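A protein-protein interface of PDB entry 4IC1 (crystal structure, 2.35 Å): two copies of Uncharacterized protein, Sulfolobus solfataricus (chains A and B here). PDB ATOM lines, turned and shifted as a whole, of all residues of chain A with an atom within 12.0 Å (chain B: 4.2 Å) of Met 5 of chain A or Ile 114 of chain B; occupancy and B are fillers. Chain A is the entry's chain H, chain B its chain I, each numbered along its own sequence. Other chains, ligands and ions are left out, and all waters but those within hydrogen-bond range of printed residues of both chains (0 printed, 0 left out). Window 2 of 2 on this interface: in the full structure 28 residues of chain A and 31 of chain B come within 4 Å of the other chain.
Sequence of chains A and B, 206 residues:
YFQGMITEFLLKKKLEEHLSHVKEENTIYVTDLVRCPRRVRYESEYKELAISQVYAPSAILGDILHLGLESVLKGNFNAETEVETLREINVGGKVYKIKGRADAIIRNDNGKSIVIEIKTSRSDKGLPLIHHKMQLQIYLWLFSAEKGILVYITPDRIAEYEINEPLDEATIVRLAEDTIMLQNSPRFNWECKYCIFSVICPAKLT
N of Ile 6 of chain A lies within hydrogen-bond range of OE2 of Glu 160 of chain B (3.1 Å). The backbone NH (N) of Met 5 of chain A lies within hydrogen-bond range of the side-chain carboxylate (OE2) of Glu 160 of chain B. The backbone NH (N) of Thr 7 of chain A is in hydrogen-bond range of the side-chain carboxylate (OE1) of Glu 160 of chain B (2.9 Å).
The side-chain amide nitrogen (NE2) of Gln 3 of chain A is in hydrogen-bond range of the side-chain hydroxyl (OG1) of Thr 7 of chain A (2.7 Å). The backbone carbonyl oxygen of Ile 114 of chain B is in hydrogen-bond range of the backbone NH of Ile 106 of chain B, at 2.9 Å.
OE1 of Glu 160 of chain B touches C of Gly 4 of chain A (3.5 Å). Met 5 of chain A touches Phe 77 of chain B (O to CZ, 3.9 Å). CE of Met 5 of chain A touches CD1 of Ile 114 of chain B, at 3.7 Å. Ile 6 of chain A touches Ile 116 of chain B (CD1 to CD1, 3.1 Å). Phe 9 of chain A touches Phe 77 of chain B.
Of chain B, only Phe 77 (3.9 Å), Ile 114 (3.7 Å) and Glu 160 (3.2 Å) come within 4 Å of Met 5 of chain A. Ile 114 of chain B touches one residue of chain A. No residue of chain A comes within 4 Å of Ile 106 of chain B. No residue of chain A comes within 4 Å of Ser 113 of chain B. No residue of chain A comes within 4 Å of Val 115 of chain B. Printed residues of chain A within 4 Å of Ile 116 of chain B: Ile 6 (3.1 Å). No residue of chain A comes within 4 Å of Lys 147 of chain B. Printed residues of chain A within 4 Å of Phe 77 of chain B: Met 5 (3.9 Å) and Phe 9 (3.7 Å). Printed residues of chain B within 4 Å of Gly 4 of chain A: Glu 160 (3.5 Å). Of the printed residues of chain A, Glu 160 of chain B touches Gly 4, Met 5, Ile 6 and Thr 7. Phe 2 of chain A touches none of the printed residues of chain B.
Printed residues of chain A that touch a printed residue of chain B: Gly 4, Met 5, Ile 6, Thr 7 and Phe 9. Hydrophobic or aromatic side chains of chain A within 4 Å of the printed part of chain B: Met 5, Ile 6 and Phe 9. Of the 9 printed residues of chain B, 4 touch a printed residue of chain A.
No position is printed for both chains. Of the 8 pairs that touch across the chains among the printed residues, none has its exchanged pair printed and touching as well.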
ATOM      1  N   TYR A   1      23.007  13.583 -10.506  1.00  0.00           N
ATOM      2  CA  TYR A   1      23.144  12.606  -9.390  1.00  0.00           C
ATOM      3  C   TYR A   1      23.714  11.222  -9.800  1.00  0.00           C
ATOM      4  O   TYR A   1      24.170  10.485  -8.927  1.00  0.00           O
ATOM      5  CB  TYR A   1      21.782  12.414  -8.671  1.00  0.00           C
ATOM      6  N   PHE A   2      23.672  10.843 -11.073  1.00  0.00           N
ATOM      7  CA  PHE A   2      24.350   9.613 -11.471  1.00  0.00           C
ATOM      8  C   PHE A   2      25.864   9.816 -11.487  1.00  0.00           C
ATOM      9  O   PHE A   2      26.596   9.095 -10.805  1.00  0.00           O
ATOM     10  CB  PHE A   2      23.941   9.119 -12.848  1.00  0.00           C
ATOM     11  CG  PHE A   2      25.006   8.266 -13.521  1.00  0.00           C
ATOM     12  CD1 PHE A   2      25.368   7.035 -12.996  1.00  0.00           C
ATOM     13  CD2 PHE A   2      25.652   8.705 -14.667  1.00  0.00           C
ATOM     14  CE1 PHE A   2      26.348   6.243 -13.624  1.00  0.00           C
ATOM     15  CE2 PHE A   2      26.625   7.932 -15.291  1.00  0.00           C
ATOM     16  CZ  PHE A   2      26.975   6.698 -14.772  1.00  0.00           C
ATOM     17  N   GLN A   3      26.312  10.757 -12.325  1.00  0.00           N
ATOM     18  CA  GLN A   3      27.715  11.167 -12.390  1.00  0.00           C
ATOM     19  C   GLN A   3      28.042  12.129 -11.251  1.00  0.00           C
ATOM     20  O   GLN A   3      29.107  12.026 -10.620  1.00  0.00           O
ATOM     21  CB  GLN A   3      28.037  11.859 -13.718  1.00  0.00           C
ATOM     22  CG  GLN A   3      29.376  12.651 -13.691  1.00  0.00           C
ATOM     23  CD  GLN A   3      30.624  11.750 -13.473  1.00  0.00           C
ATOM     24  OE1 GLN A   3      30.652  10.624 -13.932  1.00  0.00           O
ATOM     25  NE2 GLN A   3      31.646  12.266 -12.787  1.00  0.00           N
ATOM     26  N   GLY A   4      27.129  13.078 -11.009  1.00  0.00           N
ATOM     27  CA  GLY A   4      27.343  14.088 -10.003  1.00  0.00           C
ATOM     28  C   GLY A   4      27.100  15.459 -10.575  1.00  0.00           C
ATOM     29  O   GLY A   4      27.442  15.733 -11.717  1.00  0.00           O
ATOM     30  N   MET A   5      26.536  16.324  -9.740  1.00  0.00           N
ATOM     31  CA  MET A   5      26.093  17.678 -10.141  1.00  0.00           C
ATOM     32  C   MET A   5      27.235  18.474 -10.730  1.00  0.00           C
ATOM     33  O   MET A   5      27.154  18.923 -11.875  1.00  0.00           O
ATOM     34  CB  MET A   5      25.481  18.411  -8.937  1.00  0.00           C
ATOM     35  CG  MET A   5      24.482  19.493  -9.280  1.00  0.00           C
ATOM     36  SD  MET A   5      24.140  20.522  -7.682  1.00  0.00           S
ATOM     37  CE  MET A   5      22.691  19.391  -6.994  1.00  0.00           C
ATOM     38  N   ILE A   6      28.324  18.611  -9.979  1.00  0.00           N
ATOM     39  CA  ILE A   6      29.442  19.438 -10.444  1.00  0.00           C
ATOM     40  C   ILE A   6      30.120  18.840 -11.660  1.00  0.00           C
ATOM     41  O   ILE A   6      30.267  19.496 -12.697  1.00  0.00           O
ATOM     42  CB  ILE A   6      30.508  19.668  -9.364  1.00  0.00           C
ATOM     43  CG1 ILE A   6      29.967  20.532  -8.228  1.00  0.00           C
ATOM     44  CG2 ILE A   6      31.694  20.357  -9.968  1.00  0.00           C
ATOM     45  CD1 ILE A   6      29.377  19.760  -7.049  1.00  0.00           C
ATOM     46  N   THR A   7      30.511  17.578 -11.557  1.00  0.00           N
ATOM     47  CA  THR A   7      31.348  16.999 -12.618  1.00  0.00           C
ATOM     48  C   THR A   7      30.606  16.907 -13.937  1.00  0.00           C
ATOM     49  O   THR A   7      31.141  17.295 -14.968  1.00  0.00           O
ATOM     50  CB  THR A   7      31.990  15.676 -12.201  1.00  0.00           C
ATOM     51  OG1 THR A   7      30.983  14.712 -11.877  1.00  0.00           O
ATOM     52  CG2 THR A   7      32.898  15.927 -10.981  1.00  0.00           C
ATOM     53  N   GLU A   8      29.365  16.437 -13.888  1.00  0.00           N
ATOM     54  CA  GLU A   8      28.498  16.446 -15.062  1.00  0.00           C
ATOM     55  C   GLU A   8      28.628  17.771 -15.830  1.00  0.00           C
ATOM     56  O   GLU A   8      28.740  17.789 -17.076  1.00  0.00           O
ATOM     57  CB  GLU A   8      27.054  16.254 -14.652  1.00  0.00           C
ATOM     58  CG  GLU A   8      26.077  16.589 -15.797  1.00  0.00           C
ATOM     59  CD  GLU A   8      24.662  16.030 -15.624  1.00  0.00           C
ATOM     60  OE1 GLU A   8      24.426  15.167 -14.761  1.00  0.00           O
ATOM     61  OE2 GLU A   8      23.774  16.475 -16.379  1.00  0.00           O
ATOM     62  N   PHE A   9      28.606  18.872 -15.080  1.00  0.00           N
ATOM     63  CA  PHE A   9      28.650  20.208 -15.691  1.00  0.00           C
ATOM     64  C   PHE A   9      30.026  20.506 -16.244  1.00  0.00           C
ATOM     65  O   PHE A   9      30.156  21.084 -17.344  1.00  0.00           O
ATOM     66  CB  PHE A   9      28.241  21.334 -14.693  1.00  0.00           C
ATOM     67  CG  PHE A   9      28.199  22.704 -15.322  1.00  0.00           C
ATOM     68  CD1 PHE A   9      27.085  23.110 -16.064  1.00  0.00           C
ATOM     69  CD2 PHE A   9      29.296  23.564 -15.217  1.00  0.00           C
ATOM     70  CE1 PHE A   9      27.060  24.357 -16.677  1.00  0.00           C
ATOM     71  CE2 PHE A   9      29.303  24.792 -15.820  1.00  0.00           C
ATOM     72  CZ  PHE A   9      28.183  25.208 -16.562  1.00  0.00           C
ATOM     73  N   LEU A  10      31.049  20.148 -15.474  1.00  0.00           N
ATOM     74  CA  LEU A  10      32.411  20.369 -15.922  1.00  0.00           C
ATOM     75  C   LEU A  10      32.720  19.604 -17.203  1.00  0.00           C
ATOM     76  O   LEU A  10      33.408  20.120 -18.095  1.00  0.00           O
ATOM     77  CB  LEU A  10      33.392  20.015 -14.818  1.00  0.00           C
ATOM     78  CG  LEU A  10      33.327  20.851 -13.534  1.00  0.00           C
ATOM     79  CD1 LEU A  10      34.394  20.397 -12.577  1.00  0.00           C
ATOM     80  CD2 LEU A  10      33.497  22.343 -13.860  1.00  0.00           C
ATOM     81  N   LEU A  11      32.161  18.397 -17.318  1.00  0.00           N
ATOM     82  CA  LEU A  11      32.386  17.554 -18.481  1.00  0.00           C
ATOM     83  C   LEU A  11      31.642  18.082 -19.697  1.00  0.00           C
ATOM     84  O   LEU A  11      32.212  18.232 -20.764  1.00  0.00           O
ATOM     85  CB  LEU A  11      31.988  16.105 -18.168  1.00  0.00           C
ATOM     86  CG  LEU A  11      32.870  15.399 -17.099  1.00  0.00           C
ATOM     87  CD1 LEU A  11      32.305  14.014 -16.722  1.00  0.00           C
ATOM     88  CD2 LEU A  11      34.341  15.278 -17.470  1.00  0.00           C
ATOM     89  N   LYS A  12      30.368  18.401 -19.509  1.00  0.00           N
ATOM     90  CA  LYS A  12      29.533  19.110 -20.503  1.00  0.00           C
ATOM     91  C   LYS A  12      30.188  20.361 -21.126  1.00  0.00           C
ATOM     92  O   LYS A  12      30.273  20.484 -22.365  1.00  0.00           O
ATOM     93  CB  LYS A  12      28.215  19.524 -19.820  1.00  0.00           C
ATOM     94  CG  LYS A  12      27.109  20.007 -20.752  1.00  0.00           C
ATOM     95  CD  LYS A  12      25.759  20.202 -19.983  1.00  0.00           C
ATOM     96  CE  LYS A  12      25.564  21.642 -19.457  1.00  0.00           C
ATOM     97  NZ  LYS A  12      25.442  22.708 -20.543  1.00  0.00           N
ATOM     98  N   LYS A  13      30.623  21.287 -20.270  1.00  0.00           N
ATOM     99  CA  LYS A  13      31.300  22.512 -20.731  1.00  0.00           C
ATOM    100  C   LYS A  13      32.658  22.211 -21.344  1.00  0.00           C
ATOM    101  O   LYS A  13      33.117  22.958 -22.220  1.00  0.00           O
ATOM    102  CB  LYS A  13      31.472  23.542 -19.586  1.00  0.00           C
ATOM    103  N   LYS A  14      33.334  21.133 -20.909  1.00  0.00           N
ATOM    104  CA  LYS A  14      34.615  20.831 -21.527  1.00  0.00           C
ATOM    105  C   LYS A  14      34.399  20.297 -22.910  1.00  0.00           C
ATOM    106  O   LYS A  14      35.125  20.650 -23.847  1.00  0.00           O
ATOM    107  CB  LYS A  14      35.498  19.904 -20.703  1.00  0.00           C
ATOM    108  CG  LYS A  14      36.899  19.895 -21.305  1.00  0.00           C
ATOM    109  CD  LYS A  14      38.016  19.634 -20.315  1.00  0.00           C
ATOM    110  CE  LYS A  14      39.293  19.181 -21.045  1.00  0.00           C
ATOM    111  NZ  LYS A  14      40.008  20.217 -21.860  1.00  0.00           N
ATOM    112  N   ILE A  60      41.445  18.382 -17.358  1.00  0.00           N
ATOM    113  CA  ILE A  60      40.453  19.082 -16.561  1.00  0.00           C
ATOM    114  C   ILE A  60      41.093  19.864 -15.451  1.00  0.00           C
ATOM    115  O   ILE A  60      40.859  21.043 -15.313  1.00  0.00           O
ATOM    116  CB  ILE A  60      39.416  18.119 -15.992  1.00  0.00           C
ATOM    117  CG1 ILE A  60      38.637  17.475 -17.149  1.00  0.00           C
ATOM    118  CG2 ILE A  60      38.527  18.822 -15.007  1.00  0.00           C
ATOM    119  CD1 ILE A  60      37.758  16.322 -16.733  1.00  0.00           C
ATOM    120  N   ILE A  64      41.185  24.200 -15.234  1.00  0.00           N
ATOM    121  CA  ILE A  64      40.759  24.890 -14.062  1.00  0.00           C
ATOM    122  C   ILE A  64      41.879  25.729 -13.527  1.00  0.00           C
ATOM    123  O   ILE A  64      41.659  26.909 -13.200  1.00  0.00           O
ATOM    124  CB  ILE A  64      40.300  23.951 -13.022  1.00  0.00           C
ATOM    125  CG1 ILE A  64      39.017  23.284 -13.474  1.00  0.00           C
ATOM    126  CG2 ILE A  64      40.044  24.666 -11.755  1.00  0.00           C
ATOM    127  CD1 ILE A  64      38.518  22.235 -12.517  1.00  0.00           C
ATOM    128  N   PHE B  77      25.917  27.764 -10.848  1.00  0.00           N
ATOM    129  CA  PHE B  77      25.272  27.099  -9.708  1.00  0.00           C
ATOM    130  C   PHE B  77      24.720  28.131  -8.737  1.00  0.00           C
ATOM    131  O   PHE B  77      24.027  27.768  -7.792  1.00  0.00           O
ATOM    132  CB  PHE B  77      26.241  26.127  -8.997  1.00  0.00           C
ATOM    133  CG  PHE B  77      26.621  24.938  -9.841  1.00  0.00           C
ATOM    134  CD1 PHE B  77      25.813  23.803  -9.874  1.00  0.00           C
ATOM    135  CD2 PHE B  77      27.758  24.975 -10.641  1.00  0.00           C
ATOM    136  CE1 PHE B  77      26.133  22.719 -10.677  1.00  0.00           C
ATOM    137  CE2 PHE B  77      28.088  23.898 -11.433  1.00  0.00           C
ATOM    138  CZ  PHE B  77      27.273  22.763 -11.449  1.00  0.00           C
ATOM    139  N   ILE B 105      28.480  27.168  -1.026  1.00  0.00           N
ATOM    140  CA  ILE B 105      27.131  26.778  -0.547  1.00  0.00           C
ATOM    141  C   ILE B 105      26.053  27.194  -1.555  1.00  0.00           C
ATOM    142  O   ILE B 105      26.178  28.219  -2.228  1.00  0.00           O
ATOM    143  CB  ILE B 105      26.809  27.403   0.846  1.00  0.00           C
ATOM    144  CG1 ILE B 105      27.911  27.085   1.852  1.00  0.00           C
ATOM    145  CG2 ILE B 105      25.468  26.909   1.402  1.00  0.00           C
ATOM    146  CD1 ILE B 105      27.464  27.133   3.252  1.00  0.00           C
ATOM    147  N   ILE B 106      25.008  26.380  -1.668  1.00  0.00           N
ATOM    148  CA  ILE B 106      23.872  26.678  -2.545  1.00  0.00           C
ATOM    149  C   ILE B 106      22.564  26.605  -1.769  1.00  0.00           C
ATOM    150  O   ILE B 106      22.169  25.519  -1.331  1.00  0.00           O
ATOM    151  CB  ILE B 106      23.744  25.667  -3.671  1.00  0.00           C
ATOM    152  CG1 ILE B 106      24.991  25.674  -4.557  1.00  0.00           C
ATOM    153  CG2 ILE B 106      22.453  25.959  -4.476  1.00  0.00           C
ATOM    154  CD1 ILE B 106      24.957  24.581  -5.623  1.00  0.00           C
ATOM    155  N   SER B 113      19.538  23.501   1.530  1.00  0.00           N
ATOM    156  CA  SER B 113      20.854  23.908   0.970  1.00  0.00           C
ATOM    157  C   SER B 113      21.952  22.815   0.892  1.00  0.00           C
ATOM    158  O   SER B 113      21.980  21.836   1.656  1.00  0.00           O
ATOM    159  CB  SER B 113      21.397  25.136   1.699  1.00  0.00           C
ATOM    160  OG  SER B 113      21.481  24.911   3.089  1.00  0.00           O
ATOM    161  N   ILE B 114      22.851  23.006  -0.064  1.00  0.00           N
ATOM    162  CA  ILE B 114      23.897  22.038  -0.330  1.00  0.00           C
ATOM    163  C   ILE B 114      25.250  22.706  -0.221  1.00  0.00           C
ATOM    164  O   ILE B 114      25.562  23.636  -0.953  1.00  0.00           O
ATOM    165  CB  ILE B 114      23.743  21.308  -1.703  1.00  0.00           C
ATOM    166  CG1 ILE B 114      23.521  22.263  -2.855  1.00  0.00           C
ATOM    167  CG2 ILE B 114      22.546  20.351  -1.699  1.00  0.00           C
ATOM    168  CD1 ILE B 114      22.836  21.573  -4.026  1.00  0.00           C
ATOM    169  N   VAL B 115      26.033  22.225   0.736  1.00  0.00           N
ATOM    170  CA  VAL B 115      27.389  22.708   0.964  1.00  0.00           C
ATOM    171  C   VAL B 115      28.358  21.864   0.164  1.00  0.00           C
ATOM    172  O   VAL B 115      28.211  20.646   0.047  1.00  0.00           O
ATOM    173  CB  VAL B 115      27.763  22.654   2.459  1.00  0.00           C
ATOM    174  CG1 VAL B 115      27.428  21.298   3.042  1.00  0.00           C
ATOM    175  CG2 VAL B 115      29.236  22.977   2.657  1.00  0.00           C
ATOM    176  N   ILE B 116      29.355  22.508  -0.398  1.00  0.00           N
ATOM    177  CA  ILE B 116      30.198  21.776  -1.262  1.00  0.00           C
ATOM    178  C   ILE B 116      31.690  22.029  -0.986  1.00  0.00           C
ATOM    179  O   ILE B 116      32.115  23.164  -0.884  1.00  0.00           O
ATOM    180  CB  ILE B 116      29.716  21.914  -2.758  1.00  0.00           C
ATOM    181  CG1 ILE B 116      30.771  22.437  -3.694  1.00  0.00           C
ATOM    182  CG2 ILE B 116      28.437  22.726  -2.889  1.00  0.00           C
ATOM    183  CD1 ILE B 116      30.546  21.882  -5.055  1.00  0.00           C
ATOM    184  N   LYS B 147      22.419  18.481   2.715  1.00  0.00           N
ATOM    185  CA  LYS B 147      23.178  17.831   1.647  1.00  0.00           C
ATOM    186  C   LYS B 147      24.611  18.395   1.565  1.00  0.00           C
ATOM    187  O   LYS B 147      24.825  19.603   1.769  1.00  0.00           O
ATOM    188  CB  LYS B 147      22.441  17.969   0.298  1.00  0.00           C
ATOM    189  N   GLU B 160      33.244  12.473  -7.380  1.00  0.00           N
ATOM    190  CA  GLU B 160      32.283  13.234  -6.647  1.00  0.00           C
ATOM    191  C   GLU B 160      31.426  12.343  -5.753  1.00  0.00           C
ATOM    192  O   GLU B 160      30.836  11.376  -6.217  1.00  0.00           O
ATOM    193  CB  GLU B 160      31.404  13.988  -7.650  1.00  0.00           C
ATOM    194  CG  GLU B 160      30.433  14.967  -7.010  1.00  0.00           C
ATOM    195  CD  GLU B 160      29.797  15.955  -8.016  1.00  0.00           C
ATOM    196  OE1 GLU B 160      30.246  15.984  -9.205  1.00  0.00           O
ATOM    197  OE2 GLU B 160      28.839  16.688  -7.605  1.00  0.00           O
